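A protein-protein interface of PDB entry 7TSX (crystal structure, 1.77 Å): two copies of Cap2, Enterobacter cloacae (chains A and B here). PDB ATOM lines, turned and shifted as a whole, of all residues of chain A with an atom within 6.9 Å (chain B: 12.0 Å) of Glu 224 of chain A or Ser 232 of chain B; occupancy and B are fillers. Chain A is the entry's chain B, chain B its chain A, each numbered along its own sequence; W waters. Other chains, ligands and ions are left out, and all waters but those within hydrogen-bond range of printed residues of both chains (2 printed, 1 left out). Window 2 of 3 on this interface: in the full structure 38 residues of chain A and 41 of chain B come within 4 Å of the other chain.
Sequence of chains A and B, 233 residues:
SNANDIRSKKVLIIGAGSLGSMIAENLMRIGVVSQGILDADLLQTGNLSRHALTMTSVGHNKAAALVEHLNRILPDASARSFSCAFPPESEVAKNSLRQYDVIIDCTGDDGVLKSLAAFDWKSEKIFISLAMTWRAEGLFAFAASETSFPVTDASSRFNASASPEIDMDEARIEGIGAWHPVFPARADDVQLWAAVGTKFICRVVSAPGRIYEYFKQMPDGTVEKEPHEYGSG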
ATOM      1  N   TRP A 193       1.935  11.281   0.321  1.00  0.00           N
ATOM      2  CA  TRP A 193       1.474  12.645   0.073  1.00  0.00           C
ATOM      3  C   TRP A 193       2.561  13.503  -0.574  1.00  0.00           C
ATOM      4  O   TRP A 193       2.253  14.411  -1.354  1.00  0.00           O
ATOM      5  CB  TRP A 193       0.969  13.275   1.374  1.00  0.00           C
ATOM      6  CG  TRP A 193      -0.303  12.689   1.880  1.00  0.00           C
ATOM      7  CD1 TRP A 193      -0.577  12.341   3.170  1.00  0.00           C
ATOM      8  CD2 TRP A 193      -1.503  12.395   1.123  1.00  0.00           C
ATOM      9  NE1 TRP A 193      -1.855  11.847   3.261  1.00  0.00           N
ATOM     10  CE2 TRP A 193      -2.441  11.868   2.022  1.00  0.00           C
ATOM     11  CE3 TRP A 193      -1.862  12.528  -0.215  1.00  0.00           C
ATOM     12  CZ2 TRP A 193      -3.712  11.462   1.622  1.00  0.00           C
ATOM     13  CZ3 TRP A 193      -3.105  12.114  -0.617  1.00  0.00           C
ATOM     14  CH2 TRP A 193      -4.027  11.595   0.300  1.00  0.00           C
ATOM     15  N   TYR A 214      -8.463  18.550  -2.460  1.00  0.00           N
ATOM     16  CA  TYR A 214      -8.317  17.841  -1.195  1.00  0.00           C
ATOM     17  C   TYR A 214      -8.319  16.345  -1.474  1.00  0.00           C
ATOM     18  O   TYR A 214      -9.292  15.814  -2.022  1.00  0.00           O
ATOM     19  CB  TYR A 214      -9.440  18.206  -0.226  1.00  0.00           C
ATOM     20  CG  TYR A 214      -9.304  17.521   1.111  1.00  0.00           C
ATOM     21  CD1 TYR A 214      -8.402  17.986   2.057  1.00  0.00           C
ATOM     22  CD2 TYR A 214     -10.073  16.412   1.428  1.00  0.00           C
ATOM     23  CE1 TYR A 214      -8.269  17.364   3.288  1.00  0.00           C
ATOM     24  CE2 TYR A 214      -9.952  15.785   2.656  1.00  0.00           C
ATOM     25  CZ  TYR A 214      -9.052  16.268   3.579  1.00  0.00           C
ATOM     26  OH  TYR A 214      -8.926  15.656   4.801  1.00  0.00           O
ATOM     27  N   PHE A 215      -7.244  15.671  -1.078  1.00  0.00           N
ATOM     28  CA  PHE A 215      -7.066  14.243  -1.290  1.00  0.00           C
ATOM     29  C   PHE A 215      -7.241  13.500   0.027  1.00  0.00           C
ATOM     30  O   PHE A 215      -6.875  14.004   1.093  1.00  0.00           O
ATOM     31  CB  PHE A 215      -5.675  13.934  -1.857  1.00  0.00           C
ATOM     32  CG  PHE A 215      -5.419  14.539  -3.211  1.00  0.00           C
ATOM     33  CD1 PHE A 215      -4.924  15.823  -3.326  1.00  0.00           C
ATOM     34  CD2 PHE A 215      -5.664  13.816  -4.365  1.00  0.00           C
ATOM     35  CE1 PHE A 215      -4.678  16.371  -4.572  1.00  0.00           C
ATOM     36  CE2 PHE A 215      -5.422  14.361  -5.605  1.00  0.00           C
ATOM     37  CZ  PHE A 215      -4.925  15.632  -5.709  1.00  0.00           C
ATOM     38  N   LYS A 216      -7.800  12.292  -0.060  1.00  0.00           N
ATOM     39  CA  LYS A 216      -7.949  11.389   1.078  1.00  0.00           C
ATOM     40  C   LYS A 216      -7.377  10.020   0.713  1.00  0.00           C
ATOM     41  O   LYS A 216      -7.591   9.523  -0.397  1.00  0.00           O
ATOM     42  CB  LYS A 216      -9.417  11.264   1.484  1.00  0.00           C
ATOM     43  CG  LYS A 216      -9.677  10.396   2.709  1.00  0.00           C
ATOM     44  CD  LYS A 216     -11.174  10.076   2.848  1.00  0.00           C
ATOM     45  CE  LYS A 216     -11.385   8.763   3.605  1.00  0.00           C
ATOM     46  NZ  LYS A 216     -12.808   8.303   3.561  1.00  0.00           N
ATOM     47  N   GLN A 217      -6.639   9.409   1.638  1.00  0.00           N
ATOM     48  CA  GLN A 217      -6.102   8.071   1.412  1.00  0.00           C
ATOM     49  C   GLN A 217      -6.946   7.022   2.129  1.00  0.00           C
ATOM     50  O   GLN A 217      -7.465   7.261   3.225  1.00  0.00           O
ATOM     51  CB  GLN A 217      -4.638   7.970   1.858  1.00  0.00           C
ATOM     52  CG  GLN A 217      -4.405   8.119   3.344  1.00  0.00           C
ATOM     53  CD  GLN A 217      -3.043   7.563   3.769  1.00  0.00           C
ATOM     54  OE1 GLN A 217      -2.559   6.587   3.203  1.00  0.00           O
ATOM     55  NE2 GLN A 217      -2.424   8.190   4.756  1.00  0.00           N
ATOM     56  N   MET A 218      -7.109   5.876   1.484  1.00  0.00           N
ATOM     57  CA  MET A 218      -7.803   4.737   2.069  1.00  0.00           C
ATOM     58  C   MET A 218      -6.798   3.820   2.742  1.00  0.00           C
ATOM     59  O   MET A 218      -5.593   3.963   2.546  1.00  0.00           O
ATOM     60  CB  MET A 218      -8.573   3.986   0.991  1.00  0.00           C
ATOM     61  CG  MET A 218      -9.495   4.838   0.162  1.00  0.00           C
ATOM     62  SD  MET A 218     -10.786   5.594   1.148  1.00  0.00           S
ATOM     63  CE  MET A 218     -10.571   7.305   0.667  1.00  0.00           C
ATOM     64  N   THR A 222      -5.068   3.443  -1.642  1.00  0.00           N
ATOM     65  CA  THR A 222      -5.763   4.141  -2.715  1.00  0.00           C
ATOM     66  C   THR A 222      -6.055   5.583  -2.296  1.00  0.00           C
ATOM     67  O   THR A 222      -6.019   5.942  -1.113  1.00  0.00           O
ATOM     68  CB  THR A 222      -7.038   3.408  -3.123  1.00  0.00           C
ATOM     69  OG1 THR A 222      -7.918   3.215  -2.009  1.00  0.00           O
ATOM     70  CG2 THR A 222      -6.668   2.051  -3.731  1.00  0.00           C
ATOM     71  N   VAL A 223      -6.288   6.432  -3.291  1.00  0.00           N
ATOM     72  CA  VAL A 223      -6.376   7.871  -3.078  1.00  0.00           C
ATOM     73  C   VAL A 223      -7.581   8.389  -3.834  1.00  0.00           C
ATOM     74  O   VAL A 223      -7.711   8.148  -5.041  1.00  0.00           O
ATOM     75  CB  VAL A 223      -5.096   8.599  -3.533  1.00  0.00           C
ATOM     76  CG1 VAL A 223      -5.265  10.138  -3.435  1.00  0.00           C
ATOM     77  CG2 VAL A 223      -3.896   8.161  -2.690  1.00  0.00           C
ATOM     78  N   GLU A 224      -8.472   9.070  -3.115  1.00  0.00           N
ATOM     79  CA  GLU A 224      -9.618   9.761  -3.684  1.00  0.00           C
ATOM     80  C   GLU A 224      -9.414  11.269  -3.594  1.00  0.00           C
ATOM     81  O   GLU A 224      -8.609  11.760  -2.804  1.00  0.00           O
ATOM     82  CB  GLU A 224     -10.906   9.365  -2.960  1.00  0.00           C
ATOM     83  CG  GLU A 224     -11.393   7.957  -3.275  1.00  0.00           C
ATOM     84  CD  GLU A 224     -12.766   7.672  -2.693  1.00  0.00           C
ATOM     85  OE1 GLU A 224     -13.161   8.371  -1.735  1.00  0.00           O
ATOM     86  OE2 GLU A 224     -13.447   6.753  -3.195  1.00  0.00           O
ATOM     87  N   LYS A 225     -10.176  12.009  -4.397  1.00  0.00           N
ATOM     88  CA  LYS A 225      -9.935  13.431  -4.583  1.00  0.00           C
ATOM     89  C   LYS A 225     -11.251  14.185  -4.591  1.00  0.00           C
ATOM     90  O   LYS A 225     -12.257  13.683  -5.101  1.00  0.00           O
ATOM     91  CB  LYS A 225      -9.183  13.678  -5.900  1.00  0.00           C
ATOM     92  CG  LYS A 225      -9.132  15.108  -6.367  1.00  0.00           C
ATOM     93  CD  LYS A 225      -8.788  15.151  -7.865  1.00  0.00           C
ATOM     94  CE  LYS A 225      -8.343  16.536  -8.307  1.00  0.00           C
ATOM     95  NZ  LYS A 225      -7.707  16.500  -9.660  1.00  0.00           N
ATOM     96  N   GLU A 226     -11.223  15.398  -4.043  1.00  0.00           N
ATOM     97  CA  GLU A 226     -12.338  16.339  -4.126  1.00  0.00           C
ATOM     98  C   GLU A 226     -11.780  17.706  -4.515  1.00  0.00           C
ATOM     99  O   GLU A 226     -11.150  18.387  -3.691  1.00  0.00           O
ATOM    100  CB  GLU A 226     -13.089  16.414  -2.804  1.00  0.00           C
ATOM    101  CG  GLU A 226     -14.486  15.807  -2.838  1.00  0.00           C
ATOM    102  CD  GLU A 226     -15.380  16.432  -3.892  1.00  0.00           C
ATOM    103  OE1 GLU A 226     -15.273  17.655  -4.128  1.00  0.00           O
ATOM    104  OE2 GLU A 226     -16.191  15.696  -4.498  1.00  0.00           O
ATOM    105  N   LEU B 192       5.436   6.960  -4.984  1.00  0.00           N
ATOM    106  CA  LEU B 192       4.027   6.610  -4.827  1.00  0.00           C
ATOM    107  C   LEU B 192       3.864   5.106  -4.643  1.00  0.00           C
ATOM    108  O   LEU B 192       3.224   4.642  -3.686  1.00  0.00           O
ATOM    109  CB  LEU B 192       3.220   7.088  -6.031  1.00  0.00           C
ATOM    110  CG  LEU B 192       1.731   6.754  -6.011  1.00  0.00           C
ATOM    111  CD1 LEU B 192       1.012   7.596  -4.974  1.00  0.00           C
ATOM    112  CD2 LEU B 192       1.092   6.973  -7.391  1.00  0.00           C
ATOM    113  N   TRP B 193       4.445   4.322  -5.549  1.00  0.00           N
ATOM    114  CA  TRP B 193       4.254   2.877  -5.486  1.00  0.00           C
ATOM    115  C   TRP B 193       5.060   2.241  -4.361  1.00  0.00           C
ATOM    116  O   TRP B 193       4.676   1.181  -3.852  1.00  0.00           O
ATOM    117  CB  TRP B 193       4.615   2.244  -6.829  1.00  0.00           C
ATOM    118  CG  TRP B 193       3.698   2.639  -7.950  1.00  0.00           C
ATOM    119  CD1 TRP B 193       4.064   3.016  -9.214  1.00  0.00           C
ATOM    120  CD2 TRP B 193       2.262   2.695  -7.913  1.00  0.00           C
ATOM    121  NE1 TRP B 193       2.946   3.292  -9.963  1.00  0.00           N
ATOM    122  CE2 TRP B 193       1.828   3.120  -9.188  1.00  0.00           C
ATOM    123  CE3 TRP B 193       1.301   2.446  -6.921  1.00  0.00           C
ATOM    124  CZ2 TRP B 193       0.474   3.267  -9.513  1.00  0.00           C
ATOM    125  CZ3 TRP B 193      -0.057   2.601  -7.245  1.00  0.00           C
ATOM    126  CH2 TRP B 193      -0.450   3.028  -8.525  1.00  0.00           C
ATOM    127  N   VAL B 196       2.558   2.784  -1.496  1.00  0.00           N
ATOM    128  CA  VAL B 196       1.469   1.819  -1.606  1.00  0.00           C
ATOM    129  C   VAL B 196       1.991   0.412  -1.337  1.00  0.00           C
ATOM    130  O   VAL B 196       1.331  -0.404  -0.672  1.00  0.00           O
ATOM    131  CB  VAL B 196       0.809   1.918  -2.996  1.00  0.00           C
ATOM    132  CG1 VAL B 196      -0.171   0.766  -3.203  1.00  0.00           C
ATOM    133  CG2 VAL B 196       0.125   3.264  -3.179  1.00  0.00           C
ATOM    134  N   LYS B 199       2.570  -0.213   2.357  1.00  0.00           N
ATOM    135  CA  LYS B 199       1.293  -0.490   2.998  1.00  0.00           C
ATOM    136  C   LYS B 199       0.834  -1.906   2.703  1.00  0.00           C
ATOM    137  O   LYS B 199       0.314  -2.591   3.591  1.00  0.00           O
ATOM    138  CB  LYS B 199       0.234   0.518   2.537  1.00  0.00           C
ATOM    139  CG  LYS B 199       0.442   1.919   3.121  1.00  0.00           C
ATOM    140  CD  LYS B 199      -0.439   2.942   2.400  1.00  0.00           C
ATOM    141  CE  LYS B 199      -0.190   4.346   2.932  1.00  0.00           C
ATOM    142  NZ  LYS B 199      -0.180   4.402   4.417  1.00  0.00           N
ATOM    143  N   PHE B 215      -2.825  -2.012  -8.671  1.00  0.00           N
ATOM    144  CA  PHE B 215      -3.095  -0.599  -8.461  1.00  0.00           C
ATOM    145  C   PHE B 215      -2.814   0.183  -9.735  1.00  0.00           C
ATOM    146  O   PHE B 215      -1.944  -0.188 -10.522  1.00  0.00           O
ATOM    147  CB  PHE B 215      -2.225  -0.040  -7.339  1.00  0.00           C
ATOM    148  CG  PHE B 215      -2.501  -0.637  -5.986  1.00  0.00           C
ATOM    149  CD1 PHE B 215      -1.902  -1.825  -5.610  1.00  0.00           C
ATOM    150  CD2 PHE B 215      -3.344   0.000  -5.087  1.00  0.00           C
ATOM    151  CE1 PHE B 215      -2.130  -2.373  -4.367  1.00  0.00           C
ATOM    152  CE2 PHE B 215      -3.573  -0.534  -3.838  1.00  0.00           C
ATOM    153  CZ  PHE B 215      -2.970  -1.731  -3.476  1.00  0.00           C
ATOM    154  N   LYS B 216      -3.534   1.291  -9.907  1.00  0.00           N
ATOM    155  CA  LYS B 216      -3.411   2.165 -11.064  1.00  0.00           C
ATOM    156  C   LYS B 216      -3.499   3.610 -10.597  1.00  0.00           C
ATOM    157  O   LYS B 216      -4.398   3.960  -9.826  1.00  0.00           O
ATOM    158  CB  LYS B 216      -4.524   1.849 -12.084  1.00  0.00           C
ATOM    159  CG  LYS B 216      -4.484   2.660 -13.359  1.00  0.00           C
ATOM    160  CD  LYS B 216      -5.755   2.421 -14.193  1.00  0.00           C
ATOM    161  CE  LYS B 216      -5.788   3.309 -15.433  1.00  0.00           C
ATOM    162  NZ  LYS B 216      -7.115   3.272 -16.123  1.00  0.00           N
ATOM    163  N   GLN B 217      -2.573   4.444 -11.051  1.00  0.00           N
ATOM    164  CA  GLN B 217      -2.644   5.875 -10.800  1.00  0.00           C
ATOM    165  C   GLN B 217      -3.294   6.580 -11.979  1.00  0.00           C
ATOM    166  O   GLN B 217      -3.095   6.195 -13.137  1.00  0.00           O
ATOM    167  CB  GLN B 217      -1.262   6.470 -10.520  1.00  0.00           C
ATOM    168  CG  GLN B 217      -0.264   6.383 -11.660  1.00  0.00           C
ATOM    169  CD  GLN B 217       0.934   7.280 -11.414  1.00  0.00           C
ATOM    170  OE1 GLN B 217       0.791   8.477 -11.136  1.00  0.00           O
ATOM    171  NE2 GLN B 217       2.115   6.713 -11.510  1.00  0.00           N
ATOM    172  N   MET B 218      -4.089   7.599 -11.672  1.00  0.00           N
ATOM    173  CA  MET B 218      -4.894   8.303 -12.655  1.00  0.00           C
ATOM    174  C   MET B 218      -4.339   9.692 -12.930  1.00  0.00           C
ATOM    175  O   MET B 218      -3.592  10.255 -12.119  1.00  0.00           O
ATOM    176  CB  MET B 218      -6.351   8.432 -12.185  1.00  0.00           C
ATOM    177  CG  MET B 218      -6.993   7.143 -11.690  1.00  0.00           C
ATOM    178  SD  MET B 218      -6.948   5.811 -12.893  1.00  0.00           S
ATOM    179  CE  MET B 218      -7.511   6.641 -14.371  1.00  0.00           C
ATOM    180  N   PRO B 219      -4.672  10.272 -14.086  1.00  0.00           N
ATOM    181  CA  PRO B 219      -4.174  11.627 -14.391  1.00  0.00           C
ATOM    182  C   PRO B 219      -4.595  12.684 -13.379  1.00  0.00           C
ATOM    183  O   PRO B 219      -3.861  13.660 -13.182  1.00  0.00           O
ATOM    184  CB  PRO B 219      -4.766  11.922 -15.779  1.00  0.00           C
ATOM    185  CG  PRO B 219      -5.032  10.567 -16.384  1.00  0.00           C
ATOM    186  CD  PRO B 219      -5.427   9.681 -15.212  1.00  0.00           C
ATOM    187  N   ASP B 220      -5.763  12.541 -12.748  1.00  0.00           N
ATOM    188  CA  ASP B 220      -6.219  13.535 -11.778  1.00  0.00           C
ATOM    189  C   ASP B 220      -5.556  13.379 -10.410  1.00  0.00           C
ATOM    190  O   ASP B 220      -5.947  14.076  -9.467  1.00  0.00           O
ATOM    191  CB  ASP B 220      -7.740  13.480 -11.629  1.00  0.00           C
ATOM    192  CG  ASP B 220      -8.231  12.169 -11.056  1.00  0.00           C
ATOM    193  OD1 ASP B 220      -7.402  11.268 -10.813  1.00  0.00           O
ATOM    194  OD2 ASP B 220      -9.462  12.040 -10.853  1.00  0.00           O
ATOM    195  N   GLY B 221      -4.579  12.485 -10.280  1.00  0.00           N
ATOM    196  CA  GLY B 221      -3.845  12.304  -9.042  1.00  0.00           C
ATOM    197  C   GLY B 221      -4.339  11.181  -8.151  1.00  0.00           C
ATOM    198  O   GLY B 221      -3.656  10.836  -7.173  1.00  0.00           O
ATOM    199  N   THR B 222      -5.479  10.586  -8.474  1.00  0.00           N
ATOM    200  CA  THR B 222      -6.044   9.543  -7.644  1.00  0.00           C
ATOM    201  C   THR B 222      -5.358   8.204  -7.912  1.00  0.00           C
ATOM    202  O   THR B 222      -4.583   8.046  -8.858  1.00  0.00           O
ATOM    203  CB  THR B 222      -7.543   9.439  -7.887  1.00  0.00           C
ATOM    204  OG1 THR B 222      -7.797   9.192  -9.279  1.00  0.00           O
ATOM    205  CG2 THR B 222      -8.239  10.741  -7.497  1.00  0.00           C
ATOM    206  N   VAL B 223      -5.635   7.238  -7.035  1.00  0.00           N
ATOM    207  CA  VAL B 223      -5.080   5.892  -7.118  1.00  0.00           C
ATOM    208  C   VAL B 223      -6.215   4.910  -6.880  1.00  0.00           C
ATOM    209  O   VAL B 223      -6.929   5.022  -5.876  1.00  0.00           O
ATOM    210  CB  VAL B 223      -3.953   5.667  -6.095  1.00  0.00           C
ATOM    211  CG1 VAL B 223      -3.457   4.228  -6.134  1.00  0.00           C
ATOM    212  CG2 VAL B 223      -2.791   6.642  -6.348  1.00  0.00           C
ATOM    213  N   GLU B 224      -6.380   3.961  -7.804  1.00  0.00           N
ATOM    214  CA  GLU B 224      -7.432   2.959  -7.751  1.00  0.00           C
ATOM    215  C   GLU B 224      -6.829   1.564  -7.623  1.00  0.00           C
ATOM    216  O   GLU B 224      -5.659   1.330  -7.947  1.00  0.00           O
ATOM    217  CB  GLU B 224      -8.328   3.019  -9.006  1.00  0.00           C
ATOM    218  CG  GLU B 224      -8.929   4.370  -9.281  1.00  0.00           C
ATOM    219  CD  GLU B 224      -9.694   4.406 -10.593  1.00  0.00           C
ATOM    220  OE1 GLU B 224      -9.506   3.490 -11.422  1.00  0.00           O
ATOM    221  OE2 GLU B 224     -10.486   5.349 -10.787  1.00  0.00           O
ATOM    222  N   LYS B 225      -7.643   0.625  -7.135  1.00  0.00           N
ATOM    223  CA  LYS B 225      -7.197  -0.750  -6.946  1.00  0.00           C
ATOM    224  C   LYS B 225      -8.171  -1.722  -7.592  1.00  0.00           C
ATOM    225  O   LYS B 225      -9.377  -1.476  -7.601  1.00  0.00           O
ATOM    226  CB  LYS B 225      -7.075  -1.096  -5.456  1.00  0.00           C
ATOM    227  CG  LYS B 225      -6.469  -2.457  -5.182  1.00  0.00           C
ATOM    228  CD  LYS B 225      -6.344  -2.732  -3.681  1.00  0.00           C
ATOM    229  CE  LYS B 225      -7.663  -3.178  -3.074  1.00  0.00           C
ATOM    230  NZ  LYS B 225      -7.566  -3.289  -1.593  1.00  0.00           N
ATOM    231  N   GLU B 226      -7.643  -2.833  -8.111  1.00  0.00           N
ATOM    232  CA  GLU B 226      -8.438  -3.967  -8.583  1.00  0.00           C
ATOM    233  C   GLU B 226      -8.038  -5.179  -7.752  1.00  0.00           C
ATOM    234  O   GLU B 226      -6.849  -5.548  -7.745  1.00  0.00           O
ATOM    235  CB  GLU B 226      -8.194  -4.235 -10.071  1.00  0.00           C
ATOM    236  CG  GLU B 226      -9.197  -3.578 -10.992  1.00  0.00           C
ATOM    237  CD  GLU B 226     -10.624  -4.080 -10.759  1.00  0.00           C
ATOM    238  OE1 GLU B 226     -10.821  -5.309 -10.621  1.00  0.00           O
ATOM    239  OE2 GLU B 226     -11.543  -3.235 -10.698  1.00  0.00           O
ATOM    240  N   PRO B 227      -8.956  -5.819  -7.012  1.00  0.00           N
ATOM    241  CA  PRO B 227     -10.388  -5.491  -6.932  1.00  0.00           C
ATOM    242  C   PRO B 227     -10.649  -4.278  -6.050  1.00  0.00           C
ATOM    243  O   PRO B 227      -9.891  -4.040  -5.107  1.00  0.00           O
ATOM    244  CB  PRO B 227     -11.005  -6.754  -6.330  1.00  0.00           C
ATOM    245  CG  PRO B 227      -9.884  -7.424  -5.572  1.00  0.00           C
ATOM    246  CD  PRO B 227      -8.559  -6.800  -5.984  1.00  0.00           C
ATOM    247  N   HIS B 228     -11.695  -3.522  -6.382  1.00  0.00           N
ATOM    248  CA  HIS B 228     -12.071  -2.349  -5.606  1.00  0.00           C
ATOM    249  C   HIS B 228     -12.514  -2.752  -4.206  1.00  0.00           C
ATOM    250  O   HIS B 228     -13.271  -3.709  -4.031  1.00  0.00           O
ATOM    251  CB  HIS B 228     -13.201  -1.590  -6.312  1.00  0.00           C
ATOM    252  CG  HIS B 228     -13.600  -0.325  -5.624  1.00  0.00           C
ATOM    253  ND1 HIS B 228     -12.833   0.822  -5.661  1.00  0.00           N
ATOM    254  CD2 HIS B 228     -14.682  -0.033  -4.866  1.00  0.00           C
ATOM    255  CE1 HIS B 228     -13.436   1.769  -4.964  1.00  0.00           C
ATOM    256  NE2 HIS B 228     -14.560   1.276  -4.472  1.00  0.00           N
ATOM    257  N   GLU B 229     -12.049  -2.007  -3.205  1.00  0.00           N
ATOM    258  CA  GLU B 229     -12.400  -2.332  -1.829  1.00  0.00           C
ATOM    259  C   GLU B 229     -12.974  -1.141  -1.070  1.00  0.00           C
ATOM    260  O   GLU B 229     -14.031  -1.253  -0.438  1.00  0.00           O
ATOM    261  CB  GLU B 229     -11.169  -2.879  -1.093  1.00  0.00           C
ATOM    262  CG  GLU B 229     -11.480  -3.463   0.285  1.00  0.00           C
ATOM    263  CD  GLU B 229     -10.261  -4.029   0.988  1.00  0.00           C
ATOM    264  OE1 GLU B 229      -9.191  -4.179   0.355  1.00  0.00           O
ATOM    265  OE2 GLU B 229     -10.363  -4.312   2.200  1.00  0.00           O
ATOM    266  N   TYR B 230     -12.297   0.000  -1.125  1.00  0.00           N
ATOM    267  CA  TYR B 230     -12.644   1.150  -0.303  1.00  0.00           C
ATOM    268  C   TYR B 230     -13.203   2.284  -1.151  1.00  0.00           C
ATOM    269  O   TYR B 230     -12.703   2.555  -2.246  1.00  0.00           O
ATOM    270  CB  TYR B 230     -11.420   1.657   0.467  1.00  0.00           C
ATOM    271  CG  TYR B 230     -10.976   0.745   1.579  1.00  0.00           C
ATOM    272  CD1 TYR B 230     -11.667   0.706   2.787  1.00  0.00           C
ATOM    273  CD2 TYR B 230      -9.872  -0.080   1.426  1.00  0.00           C
ATOM    274  CE1 TYR B 230     -11.262  -0.132   3.811  1.00  0.00           C
ATOM    275  CE2 TYR B 230      -9.462  -0.917   2.444  1.00  0.00           C
ATOM    276  CZ  TYR B 230     -10.167  -0.940   3.634  1.00  0.00           C
ATOM    277  OH  TYR B 230      -9.762  -1.768   4.647  1.00  0.00           O
ATOM    278  N   GLY B 231     -14.218   2.966  -0.617  1.00  0.00           N
ATOM    279  CA  GLY B 231     -14.782   4.127  -1.266  1.00  0.00           C
ATOM    280  C   GLY B 231     -15.777   3.765  -2.347  1.00  0.00           C
ATOM    281  O   GLY B 231     -16.201   2.616  -2.504  1.00  0.00           O
ATOM    282  N   SER B 232     -16.166   4.790  -3.102  1.00  0.00           N
ATOM    283  CA  SER B 232     -17.136   4.629  -4.184  1.00  0.00           C
ATOM    284  C   SER B 232     -16.514   3.945  -5.397  1.00  0.00           C
ATOM    285  O   SER B 232     -15.378   4.235  -5.774  1.00  0.00           O
ATOM    286  CB  SER B 232     -17.714   5.992  -4.587  1.00  0.00           C
ATOM    287  OG  SER B 232     -16.681   6.946  -4.761  1.00  0.00           O
HETATM  288  O   HOH W   1      -3.384   4.624   4.365  1.00  0.00           O
HETATM  289  O   HOH W   2     -10.355   3.230  -3.246  1.00  0.00           O
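Glu 224 of chain A touches two residues of chain B.
Of chain A, only Glu 224 comes within 4 Å of Ser 232 of chain B.
Phe 215 of chain A touches just one residue of chain B: Asp 220 (3.9 Å).
No residue of chain B comes within 4 Å of Lys 216 of chain A.
Of chain B, only Val 223 (3.2 Å), Glu 224 (3.9 Å) and Lys 225 (3.6 Å) come within 4 Å of Thr 222 of chain A.
Printed residues of chain B within 4 Å of Met 218 of chain A: Tyr 230 (3.7 Å).
Of the printed residues of chain A, Lys 225 of chain B touches Thr 222.
Printed residues of chain A within 4 Å of Lys 199 of chain B: Gln 217.
The nearest printed residue of chain A that does not touch Ser 232 of chain B is Met 218 of chain A (6.9 Å).
The nearest printed residue of chain A that does not touch Thr 222 of chain B is Glu 224 of chain A (4.1 Å).
The backbone carbonyl oxygen (O) of Val 223 of chain B sits at hydrogen-bond distance from the backbone NH (N) of Val 223 of chain A (3.0 Å).
The side-chain amino group (NZ) of Lys 199 of chain B sits close to the side-chain amide oxygen (OE1) of Gln 217 of chain A (3.5 Å).
N of Ser 232 of chain B sits at hydrogen-bond distance from OE2 of Glu 224 of chain A (3.4 Å).
NZ of Lys 225 of chain A is in hydrogen-bond range of O of Asp 220 of chain B, 3.0 Å away.
Among the printed residues, merely in contact across the chains: Phe 215 of chain A with Asp 220 of chain B, Met 218 of chain A with Tyr 230 of chain B, Thr 222 of chain A with Val 223 of chain B, Thr 222 of chain A with Glu 224 of chain B, Thr 222 of chain A with Lys 225 of chain B, Val 223 of chain A with Thr 222 of chain B, Glu 224 of chain A with Gly 231 of chain B and Lys 225 of chain A with Thr 222 of chain B.
Water W1 lies within hydrogen-bond range of the side-chain amide oxygen of Gln 217 of chain A (2.4 Å), the backbone carbonyl oxygen of Met 218 of chain A (2.9 Å) and the side-chain amino group of Lys 199 of chain B (3.2 Å).
Water W2 lies within hydrogen-bond range of the backbone carbonyl oxygen of Tyr 230 of chain B (2.6 Å) and the side-chain hydroxyl of Thr 222 of chain A (2.7 Å).
Of the 22 printed residues of chain B, 9 touch a printed residue of chain A.
Along chain B the printed residues that touch a printed residue of chain A span positions 199 to 232.
Hydrophobic or aromatic side chains of chain A that line the printed part of chain B: Phe 215, Met 218 and Val 223.
Among the printed residues, 12 pairs touch across the chains.
Thr 222 of chain A touches Val 223 of chain B, and with the chains exchanged Val 223 of chain A touches Thr 222 of chain B.
Thr 222 of chain A touches Glu 224 of chain B, but with the chains exchanged Glu 224 of chain A does not touch Thr 222 of chain B (4.1 Å).
Thr 222 of chain A touches Lys 225 of chain B, and with the chains exchanged Lys 225 of chain A touches Thr 222 of chain B.
Val 223 of chain B touches its own counterpart, Val 223 of chain A.
OG1 of Thr 222 of chain B lies within hydrogen-bond range of OD1 of Asp 220 of chain B, at 2.6 Å.
NE2 of His 228 of chain B lies close to O of Ser 232 of chain B (3.3 Å).
The side-chain carboxylate (OE1) of Glu 229 of chain B is in salt-bridge range of the side-chain amino group (NZ) of Lys 225 of chain B (2.7 Å).
N of Glu 224 of chain B is in hydrogen-bond range of O of Lys 216 of chain B.
A ring nitrogen (NE2) of His 228 of chain B lies within hydrogen-bond range of the backbone carbonyl oxygen (O) of Gly 231 of chain B (2.9 Å).
The backbone carbonyl oxygen (O) of Lys 216 of chain A sits at hydrogen-bond distance from the backbone NH (N) of Glu 224 of chain A (2.9 Å).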
